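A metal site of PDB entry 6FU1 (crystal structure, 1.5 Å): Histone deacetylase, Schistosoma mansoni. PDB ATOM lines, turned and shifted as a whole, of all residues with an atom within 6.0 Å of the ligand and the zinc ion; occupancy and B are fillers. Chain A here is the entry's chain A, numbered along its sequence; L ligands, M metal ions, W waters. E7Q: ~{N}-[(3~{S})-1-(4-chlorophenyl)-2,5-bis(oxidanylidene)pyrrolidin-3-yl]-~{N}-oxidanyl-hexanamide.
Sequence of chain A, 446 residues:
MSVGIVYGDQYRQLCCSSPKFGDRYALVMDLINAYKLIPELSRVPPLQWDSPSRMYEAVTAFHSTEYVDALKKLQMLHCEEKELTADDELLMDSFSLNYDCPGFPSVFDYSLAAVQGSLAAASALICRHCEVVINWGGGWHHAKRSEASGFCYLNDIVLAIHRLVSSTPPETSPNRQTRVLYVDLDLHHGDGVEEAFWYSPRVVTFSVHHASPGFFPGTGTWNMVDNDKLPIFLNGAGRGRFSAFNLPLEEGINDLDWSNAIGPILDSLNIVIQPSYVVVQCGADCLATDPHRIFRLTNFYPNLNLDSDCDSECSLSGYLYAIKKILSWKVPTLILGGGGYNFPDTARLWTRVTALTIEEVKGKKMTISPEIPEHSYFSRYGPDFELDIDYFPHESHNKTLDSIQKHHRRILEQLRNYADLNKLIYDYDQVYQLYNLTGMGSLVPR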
ATOM      1  N   PHE A  21     -21.323  -5.912 -27.209  1.00  0.00           N
ATOM      2  CA  PHE A  21     -20.203  -5.611 -26.328  1.00  0.00           C
ATOM      3  C   PHE A  21     -19.097  -4.812 -27.002  1.00  0.00           C
ATOM      4  O   PHE A  21     -18.114  -4.463 -26.342  1.00  0.00           O
ATOM      5  CB  PHE A  21     -19.645  -6.909 -25.734  1.00  0.00           C
ATOM      6  CG  PHE A  21     -20.588  -7.534 -24.757  1.00  0.00           C
ATOM      7  CD1 PHE A  21     -20.742  -6.983 -23.505  1.00  0.00           C
ATOM      8  CD2 PHE A  21     -21.353  -8.628 -25.104  1.00  0.00           C
ATOM      9  CE1 PHE A  21     -21.609  -7.532 -22.603  1.00  0.00           C
ATOM     10  CE2 PHE A  21     -22.233  -9.183 -24.204  1.00  0.00           C
ATOM     11  CZ  PHE A  21     -22.374  -8.626 -22.950  1.00  0.00           C
ATOM     12  N   ARG A  24     -15.426  -3.344 -25.677  1.00  0.00           N
ATOM     13  CA  ARG A  24     -15.202  -3.439 -24.237  1.00  0.00           C
ATOM     14  C   ARG A  24     -13.924  -4.191 -23.909  1.00  0.00           C
ATOM     15  O   ARG A  24     -13.138  -3.764 -23.048  1.00  0.00           O
ATOM     16  CB  ARG A  24     -16.400  -4.110 -23.558  1.00  0.00           C
ATOM     17  CG  ARG A  24     -16.285  -4.168 -22.047  1.00  0.00           C
ATOM     18  CD  ARG A  24     -17.443  -4.937 -21.453  1.00  0.00           C
ATOM     19  NE  ARG A  24     -17.259  -6.378 -21.636  1.00  0.00           N
ATOM     20  CZ  ARG A  24     -17.992  -7.306 -21.025  1.00  0.00           C
ATOM     21  NH1 ARG A  24     -18.972  -6.947 -20.201  1.00  0.00           N
ATOM     22  NH2 ARG A  24     -17.720  -8.586 -21.227  1.00  0.00           N
ATOM     23  N   ASP A 100     -32.809 -10.638 -28.729  1.00  0.00           N
ATOM     24  CA  ASP A 100     -31.639 -10.230 -27.958  1.00  0.00           C
ATOM     25  C   ASP A 100     -30.353 -10.936 -28.393  1.00  0.00           C
ATOM     26  O   ASP A 100     -29.265 -10.411 -28.137  1.00  0.00           O
ATOM     27  CB  ASP A 100     -31.858 -10.492 -26.468  1.00  0.00           C
ATOM     28  CG  ASP A 100     -32.920  -9.610 -25.875  1.00  0.00           C
ATOM     29  OD1 ASP A 100     -32.852  -8.378 -26.078  1.00  0.00           O
ATOM     30  OD2 ASP A 100     -33.820 -10.154 -25.207  1.00  0.00           O
ATOM     31  N   GLY A 139     -17.012 -15.947 -19.801  1.00  0.00           N
ATOM     32  CA  GLY A 139     -18.011 -15.801 -18.749  1.00  0.00           C
ATOM     33  C   GLY A 139     -19.453 -15.771 -19.198  1.00  0.00           C
ATOM     34  O   GLY A 139     -20.289 -15.160 -18.539  1.00  0.00           O
ATOM     35  N   TRP A 140     -19.790 -16.473 -20.295  1.00  0.00           N
ATOM     36  CA  TRP A 140     -21.112 -16.346 -20.922  1.00  0.00           C
ATOM     37  C   TRP A 140     -22.084 -17.390 -20.354  1.00  0.00           C
ATOM     38  O   TRP A 140     -22.486 -18.356 -21.005  1.00  0.00           O
ATOM     39  CB  TRP A 140     -20.956 -16.421 -22.442  1.00  0.00           C
ATOM     40  CG  TRP A 140     -19.958 -15.366 -22.838  1.00  0.00           C
ATOM     41  CD1 TRP A 140     -18.681 -15.584 -23.286  1.00  0.00           C
ATOM     42  CD2 TRP A 140     -20.098 -13.942 -22.675  1.00  0.00           C
ATOM     43  NE1 TRP A 140     -18.047 -14.361 -23.485  1.00  0.00           N
ATOM     44  CE2 TRP A 140     -18.888 -13.351 -23.106  1.00  0.00           C
ATOM     45  CE3 TRP A 140     -21.136 -13.109 -22.242  1.00  0.00           C
ATOM     46  CZ2 TRP A 140     -18.699 -11.969 -23.122  1.00  0.00           C
ATOM     47  CZ3 TRP A 140     -20.935 -11.741 -22.245  1.00  0.00           C
ATOM     48  CH2 TRP A 140     -19.722 -11.186 -22.676  1.00  0.00           C
ATOM     49  N   HIS A 141     -22.539 -17.104 -19.122  1.00  0.00           N
ATOM     50  CA  HIS A 141     -23.181 -18.096 -18.256  1.00  0.00           C
ATOM     51  C   HIS A 141     -24.617 -18.439 -18.638  1.00  0.00           C
ATOM     52  O   HIS A 141     -25.162 -19.381 -18.062  1.00  0.00           O
ATOM     53  CB  HIS A 141     -23.127 -17.622 -16.780  1.00  0.00           C
ATOM     54  CG  HIS A 141     -23.727 -16.270 -16.512  1.00  0.00           C
ATOM     55  ND1 HIS A 141     -23.912 -15.760 -15.233  1.00  0.00           N
ATOM     56  CD2 HIS A 141     -24.169 -15.300 -17.350  1.00  0.00           C
ATOM     57  CE1 HIS A 141     -24.434 -14.556 -15.300  1.00  0.00           C
ATOM     58  NE2 HIS A 141     -24.595 -14.244 -16.571  1.00  0.00           N
ATOM     59  N   HIS A 142     -25.239 -17.726 -19.586  1.00  0.00           N
ATOM     60  CA  HIS A 142     -26.643 -17.985 -19.882  1.00  0.00           C
ATOM     61  C   HIS A 142     -26.881 -19.000 -20.988  1.00  0.00           C
ATOM     62  O   HIS A 142     -28.013 -19.498 -21.096  1.00  0.00           O
ATOM     63  CB  HIS A 142     -27.360 -16.667 -20.286  1.00  0.00           C
ATOM     64  CG  HIS A 142     -27.486 -15.664 -19.176  1.00  0.00           C
ATOM     65  ND1 HIS A 142     -28.021 -15.970 -17.946  1.00  0.00           N
ATOM     66  CD2 HIS A 142     -27.139 -14.362 -19.119  1.00  0.00           C
ATOM     67  CE1 HIS A 142     -27.997 -14.897 -17.173  1.00  0.00           C
ATOM     68  NE2 HIS A 142     -27.470 -13.902 -17.868  1.00  0.00           N
ATOM     69  N   SER A 149     -29.116 -17.312 -25.109  1.00  0.00           N
ATOM     70  CA  SER A 149     -29.842 -16.643 -24.042  1.00  0.00           C
ATOM     71  C   SER A 149     -29.014 -15.474 -23.511  1.00  0.00           C
ATOM     72  O   SER A 149     -27.811 -15.625 -23.303  1.00  0.00           O
ATOM     73  CB  SER A 149     -30.140 -17.628 -22.911  1.00  0.00           C
ATOM     74  OG  SER A 149     -30.883 -16.994 -21.876  1.00  0.00           O
ATOM     75  N   GLY A 150     -29.643 -14.325 -23.314  1.00  0.00           N
ATOM     76  CA  GLY A 150     -28.936 -13.210 -22.697  1.00  0.00           C
ATOM     77  C   GLY A 150     -27.597 -12.843 -23.327  1.00  0.00           C
ATOM     78  O   GLY A 150     -26.604 -12.655 -22.607  1.00  0.00           O
ATOM     79  N   PHE A 151     -27.590 -12.731 -24.655  1.00  0.00           N
ATOM     80  CA  PHE A 151     -26.376 -12.397 -25.417  1.00  0.00           C
ATOM     81  C   PHE A 151     -25.290 -13.453 -25.278  1.00  0.00           C
ATOM     82  O   PHE A 151     -24.124 -13.180 -25.596  1.00  0.00           O
ATOM     83  CB  PHE A 151     -25.815 -11.017 -25.009  1.00  0.00           C
ATOM     84  CG  PHE A 151     -26.873 -10.001 -24.644  1.00  0.00           C
ATOM     85  CD1 PHE A 151     -27.971  -9.789 -25.455  1.00  0.00           C
ATOM     86  CD2 PHE A 151     -26.763  -9.271 -23.472  1.00  0.00           C
ATOM     87  CE1 PHE A 151     -28.943  -8.859 -25.103  1.00  0.00           C
ATOM     88  CE2 PHE A 151     -27.733  -8.346 -23.112  1.00  0.00           C
ATOM     89  CZ  PHE A 151     -28.825  -8.144 -23.930  1.00  0.00           C
ATOM     90  N   CYS A 152     -25.626 -14.647 -24.802  1.00  0.00           N
ATOM     91  CA  CYS A 152     -24.686 -15.753 -24.692  1.00  0.00           C
ATOM     92  C   CYS A 152     -25.052 -16.799 -25.745  1.00  0.00           C
ATOM     93  O   CYS A 152     -26.185 -17.290 -25.762  1.00  0.00           O
ATOM     94  CB  CYS A 152     -24.730 -16.388 -23.304  1.00  0.00           C
ATOM     95  SG  CYS A 152     -24.388 -15.211 -21.939  1.00  0.00           S
ATOM     96  N   ASP A 186     -22.131 -12.165 -11.113  1.00  0.00           N
ATOM     97  CA  ASP A 186     -22.894 -11.316 -12.016  1.00  0.00           C
ATOM     98  C   ASP A 186     -24.199 -10.849 -11.371  1.00  0.00           C
ATOM     99  O   ASP A 186     -24.776 -11.529 -10.516  1.00  0.00           O
ATOM    100  CB  ASP A 186     -23.191 -12.138 -13.286  1.00  0.00           C
ATOM    101  CG  ASP A 186     -23.539 -11.296 -14.483  1.00  0.00           C
ATOM    102  OD1 ASP A 186     -24.707 -10.898 -14.594  1.00  0.00           O
ATOM    103  OD2 ASP A 186     -22.673 -11.078 -15.363  1.00  0.00           O
ATOM    104  N   LEU A 187     -24.688  -9.694 -11.831  1.00  0.00           N
ATOM    105  CA  LEU A 187     -26.013  -9.236 -11.408  1.00  0.00           C
ATOM    106  C   LEU A 187     -27.100 -10.254 -11.738  1.00  0.00           C
ATOM    107  O   LEU A 187     -28.135 -10.309 -11.045  1.00  0.00           O
ATOM    108  CB  LEU A 187     -26.305  -7.901 -12.092  1.00  0.00           C
ATOM    109  CG  LEU A 187     -27.667  -7.271 -11.851  1.00  0.00           C
ATOM    110  CD1 LEU A 187     -27.774  -6.731 -10.445  1.00  0.00           C
ATOM    111  CD2 LEU A 187     -27.869  -6.143 -12.861  1.00  0.00           C
ATOM    112  N   HIS A 188     -26.916 -11.045 -12.791  1.00  0.00           N
ATOM    113  CA  HIS A 188     -27.924 -11.993 -13.248  1.00  0.00           C
ATOM    114  C   HIS A 188     -27.627 -13.407 -12.765  1.00  0.00           C
ATOM    115  O   HIS A 188     -26.468 -13.790 -12.592  1.00  0.00           O
ATOM    116  CB  HIS A 188     -28.001 -11.987 -14.777  1.00  0.00           C
ATOM    117  CG  HIS A 188     -28.358 -10.657 -15.329  1.00  0.00           C
ATOM    118  ND1 HIS A 188     -27.400  -9.692 -15.630  1.00  0.00           N
ATOM    119  CD2 HIS A 188     -29.559 -10.070 -15.551  1.00  0.00           C
ATOM    120  CE1 HIS A 188     -28.011  -8.586 -16.013  1.00  0.00           C
ATOM    121  NE2 HIS A 188     -29.316  -8.807 -16.023  1.00  0.00           N
ATOM    122  N   PHE A 216     -34.730 -10.568 -15.904  1.00  0.00           N
ATOM    123  CA  PHE A 216     -34.016 -11.656 -16.566  1.00  0.00           C
ATOM    124  C   PHE A 216     -33.018 -12.377 -15.637  1.00  0.00           C
ATOM    125  O   PHE A 216     -32.350 -11.719 -14.843  1.00  0.00           O
ATOM    126  CB  PHE A 216     -33.290 -11.088 -17.782  1.00  0.00           C
ATOM    127  CG  PHE A 216     -32.592 -12.117 -18.596  1.00  0.00           C
ATOM    128  CD1 PHE A 216     -33.248 -12.748 -19.630  1.00  0.00           C
ATOM    129  CD2 PHE A 216     -31.280 -12.464 -18.332  1.00  0.00           C
ATOM    130  CE1 PHE A 216     -32.625 -13.710 -20.384  1.00  0.00           C
ATOM    131  CE2 PHE A 216     -30.635 -13.428 -19.080  1.00  0.00           C
ATOM    132  CZ  PHE A 216     -31.309 -14.054 -20.108  1.00  0.00           C
ATOM    133  N   GLN A 281     -17.200 -16.301 -12.028  1.00  0.00           N
ATOM    134  CA  GLN A 281     -17.698 -15.377 -13.043  1.00  0.00           C
ATOM    135  C   GLN A 281     -17.813 -14.021 -12.370  1.00  0.00           C
ATOM    136  O   GLN A 281     -18.454 -13.899 -11.320  1.00  0.00           O
ATOM    137  CB  GLN A 281     -19.051 -15.868 -13.577  1.00  0.00           C
ATOM    138  CG  GLN A 281     -19.459 -15.301 -14.934  1.00  0.00           C
ATOM    139  CD  GLN A 281     -20.276 -14.043 -14.821  1.00  0.00           C
ATOM    140  OE1 GLN A 281     -20.254 -13.368 -13.789  1.00  0.00           O
ATOM    141  NE2 GLN A 281     -20.995 -13.720 -15.876  1.00  0.00           N
ATOM    142  N   GLY A 283     -18.905 -10.895 -13.624  1.00  0.00           N
ATOM    143  CA  GLY A 283     -19.633  -9.902 -14.401  1.00  0.00           C
ATOM    144  C   GLY A 283     -19.765  -8.598 -13.650  1.00  0.00           C
ATOM    145  O   GLY A 283     -20.074  -8.601 -12.457  1.00  0.00           O
ATOM    146  N   ASP A 285     -21.811  -5.974 -13.965  1.00  0.00           N
ATOM    147  CA  ASP A 285     -23.060  -5.220 -14.005  1.00  0.00           C
ATOM    148  C   ASP A 285     -23.666  -4.982 -12.616  1.00  0.00           C
ATOM    149  O   ASP A 285     -24.749  -4.387 -12.515  1.00  0.00           O
ATOM    150  CB  ASP A 285     -24.074  -5.909 -14.959  1.00  0.00           C
ATOM    151  CG  ASP A 285     -24.035  -7.445 -14.908  1.00  0.00           C
ATOM    152  OD1 ASP A 285     -23.406  -8.058 -14.028  1.00  0.00           O
ATOM    153  OD2 ASP A 285     -24.690  -8.040 -15.796  1.00  0.00           O
ATOM    154  N   HIS A 292     -27.807  -0.728 -15.765  1.00  0.00           N
ATOM    155  CA  HIS A 292     -28.922  -1.435 -15.139  1.00  0.00           C
ATOM    156  C   HIS A 292     -29.404  -0.696 -13.891  1.00  0.00           C
ATOM    157  O   HIS A 292     -30.609  -0.684 -13.595  1.00  0.00           O
ATOM    158  CB  HIS A 292     -28.521  -2.864 -14.759  1.00  0.00           C
ATOM    159  CG  HIS A 292     -28.538  -3.812 -15.913  1.00  0.00           C
ATOM    160  ND1 HIS A 292     -27.427  -4.031 -16.706  1.00  0.00           N
ATOM    161  CD2 HIS A 292     -29.520  -4.579 -16.425  1.00  0.00           C
ATOM    162  CE1 HIS A 292     -27.735  -4.910 -17.647  1.00  0.00           C
ATOM    163  NE2 HIS A 292     -29.004  -5.258 -17.506  1.00  0.00           N
ATOM    164  N   GLY A 337     -14.923 -13.028 -17.108  1.00  0.00           N
ATOM    165  CA  GLY A 337     -15.783 -11.862 -17.206  1.00  0.00           C
ATOM    166  C   GLY A 337     -17.272 -12.170 -17.177  1.00  0.00           C
ATOM    167  O   GLY A 337     -17.736 -13.074 -16.470  1.00  0.00           O
ATOM    168  N   GLY A 338     -18.017 -11.420 -17.967  1.00  0.00           N
ATOM    169  CA  GLY A 338     -19.450 -11.618 -18.058  1.00  0.00           C
ATOM    170  C   GLY A 338     -20.112 -10.311 -18.418  1.00  0.00           C
ATOM    171  O   GLY A 338     -19.661  -9.619 -19.337  1.00  0.00           O
ATOM    172  N   GLY A 339     -21.193  -9.974 -17.698  1.00  0.00           N
ATOM    173  CA  GLY A 339     -21.900  -8.732 -17.959  1.00  0.00           C
ATOM    174  C   GLY A 339     -21.057  -7.527 -17.602  1.00  0.00           C
ATOM    175  O   GLY A 339     -19.966  -7.624 -17.042  1.00  0.00           O
ATOM    176  N   GLY A 340     -21.587  -6.358 -17.935  1.00  0.00           N
ATOM    177  CA  GLY A 340     -20.875  -5.112 -17.707  1.00  0.00           C
ATOM    178  C   GLY A 340     -21.079  -4.237 -18.910  1.00  0.00           C
ATOM    179  O   GLY A 340     -20.450  -4.429 -19.956  1.00  0.00           O
ATOM    180  N   TYR A 341     -22.001  -3.279 -18.782  1.00  0.00           N
ATOM    181  CA  TYR A 341     -22.438  -2.469 -19.909  1.00  0.00           C
ATOM    182  C   TYR A 341     -21.979  -1.019 -19.823  1.00  0.00           C
ATOM    183  O   TYR A 341     -22.271  -0.233 -20.716  1.00  0.00           O
ATOM    184  CB  TYR A 341     -23.966  -2.599 -20.034  1.00  0.00           C
ATOM    185  CG  TYR A 341     -24.290  -4.078 -20.116  1.00  0.00           C
ATOM    186  CD1 TYR A 341     -24.253  -4.740 -21.334  1.00  0.00           C
ATOM    187  CD2 TYR A 341     -24.504  -4.832 -18.956  1.00  0.00           C
ATOM    188  CE1 TYR A 341     -24.473  -6.126 -21.411  1.00  0.00           C
ATOM    189  CE2 TYR A 341     -24.704  -6.227 -19.032  1.00  0.00           C
ATOM    190  CZ  TYR A 341     -24.693  -6.851 -20.255  1.00  0.00           C
ATOM    191  OH  TYR A 341     -24.903  -8.206 -20.351  1.00  0.00           O
HETATM  192  C01 E7Q L   1     -22.624 -13.566 -19.448  1.00  0.00           C
HETATM  193  C02 E7Q L   1     -22.855 -12.245 -18.848  1.00  0.00           C
HETATM  194  C03 E7Q L   1     -23.144 -11.162 -19.871  1.00  0.00           C
HETATM  195  C04 E7Q L   1     -24.347 -11.395 -20.751  1.00  0.00           C
HETATM  196  C05 E7Q L   1     -25.548 -11.871 -19.965  1.00  0.00           C
HETATM  197  C06 E7Q L   1     -25.781 -11.094 -18.692  1.00  0.00           C
HETATM  198  C10 E7Q L   1     -27.694  -9.463 -18.881  1.00  0.00           C
HETATM  199  C11 E7Q L   1     -27.946  -7.947 -19.049  1.00  0.00           C
HETATM  200  C12 E7Q L   1     -29.358  -7.923 -19.569  1.00  0.00           C
HETATM  201  C15 E7Q L   1     -30.888  -9.499 -20.781  1.00  0.00           C
HETATM  202  C16 E7Q L   1     -32.081  -8.965 -20.321  1.00  0.00           C
HETATM  203  C17 E7Q L   1     -33.287  -9.361 -20.883  1.00  0.00           C
HETATM  204  C18 E7Q L   1     -33.280 -10.301 -21.902  1.00  0.00           C
HETATM  205  C20 E7Q L   1     -32.104 -10.824 -22.388  1.00  0.00           C
HETATM  206  C21 E7Q L   1     -30.906 -10.413 -21.826  1.00  0.00           C
HETATM  207  C22 E7Q L   1     -28.623 -10.097 -19.900  1.00  0.00           C
HETATM  208  N08 E7Q L   1     -26.256  -9.828 -18.813  1.00  0.00           N
HETATM  209  N14 E7Q L   1     -29.646  -9.166 -20.135  1.00  0.00           N
HETATM  210  O07 E7Q L   1     -25.533 -11.560 -17.590  1.00  0.00           O
HETATM  211  O09 E7Q L   1     -25.512  -8.899 -18.072  1.00  0.00           O
HETATM  212  O13 E7Q L   1     -30.167  -7.006 -19.466  1.00  0.00           O
HETATM  213  O23 E7Q L   1     -28.536 -11.192 -20.417  1.00  0.00           O
HETATM  214 CL   E7Q L   1     -34.799 -10.859 -22.546  1.00  0.00          CL
HETATM  215 ZN    ZN M   1     -25.344  -9.901 -16.117  1.00  0.00          ZN
HETATM  216  O   HOH W   1     -32.342 -13.708 -24.096  1.00  0.00           O
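An oxygen (O07) of the ligand sits close to a ring nitrogen (NE2) of His 141 (3.0 Å).
A ring nitrogen (NE2) of His 142 lies close to an oxygen (O07) of the ligand.
A ring nitrogen (NE2) of His 292 lies within hydrogen-bond range of an oxygen (O13) of the ligand (2.9 Å).
The side-chain hydroxyl (OH) of Tyr 341 lies close to an oxygen (O09) of the ligand (2.5 Å).
SG of Cys 152 sits close to O of Ser 149, 3.7 Å away.
The backbone carbonyl oxygen (O) of Gly 150 lies within hydrogen-bond range of the side-chain sulfur (SG) of Cys 152 (3.4 Å).
NE2 of Gln 281 lies within hydrogen-bond range of OD2 of Asp 186, at 3.2 Å.
N of Gly 283 is in hydrogen-bond range of OE1 of Gln 281, at 2.8 Å.
OD1 of Asp 285 sits at hydrogen-bond distance from N of Leu 187 (3.0 Å).
A ring nitrogen (NE2) of His 141 is in hydrogen-bond range of a ring nitrogen (NE2) of His 142 (3.2 Å).
The backbone NH of His 142 lies within hydrogen-bond range of the side-chain sulfur of Cys 152, 3.5 Å away.
O of Gly 339 is in hydrogen-bond range of NH1 of Arg 24 (3.4 Å).
The backbone carbonyl oxygen (O) of Gly 150 sits close to an oxygen (O23) of the ligand.
OD2 of Asp 100 touches CL of the ligand (2.9 Å).
Gly 139 touches the ligand (O to C01, 3.0 Å).
Trp 140 touches the ligand.
Phe 151 touches the ligand.
Cys 152 touches the ligand (SG to C01, 3.5 Å).
Phe 216 touches the ligand (CD1 to C18, 3.3 Å).
Gln 281 touches the ligand.
C of Gly 338 touches C02 of the ligand (3.4 Å).
N of Gly 339 touches C02 of the ligand, 3.0 Å away.
Hydrophobic or aromatic side chains within 4 Å of the ligand: Trp 140, His 141, His 142, Phe 151, His 188, Phe 216, His 292 and Tyr 341.
The nearest printed residue that does not touch the ligand is Phe 21 (4.05 Å).
Within 4 Å of the zinc ion: Asp 186, His 188 and Asp 285.
The zinc ion is bound by the side-chain carboxylate of Asp 186 (1.9 Å), the side-chain carboxylate of Asp 285 (2.0 Å), a ring nitrogen (ND1) of His 188 (2.1 Å), an oxygen (O09) of the ligand (2.2 Å) and an oxygen (O07) of the ligand (2.2 Å).
The zinc ion has five donor atoms within binding distance.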
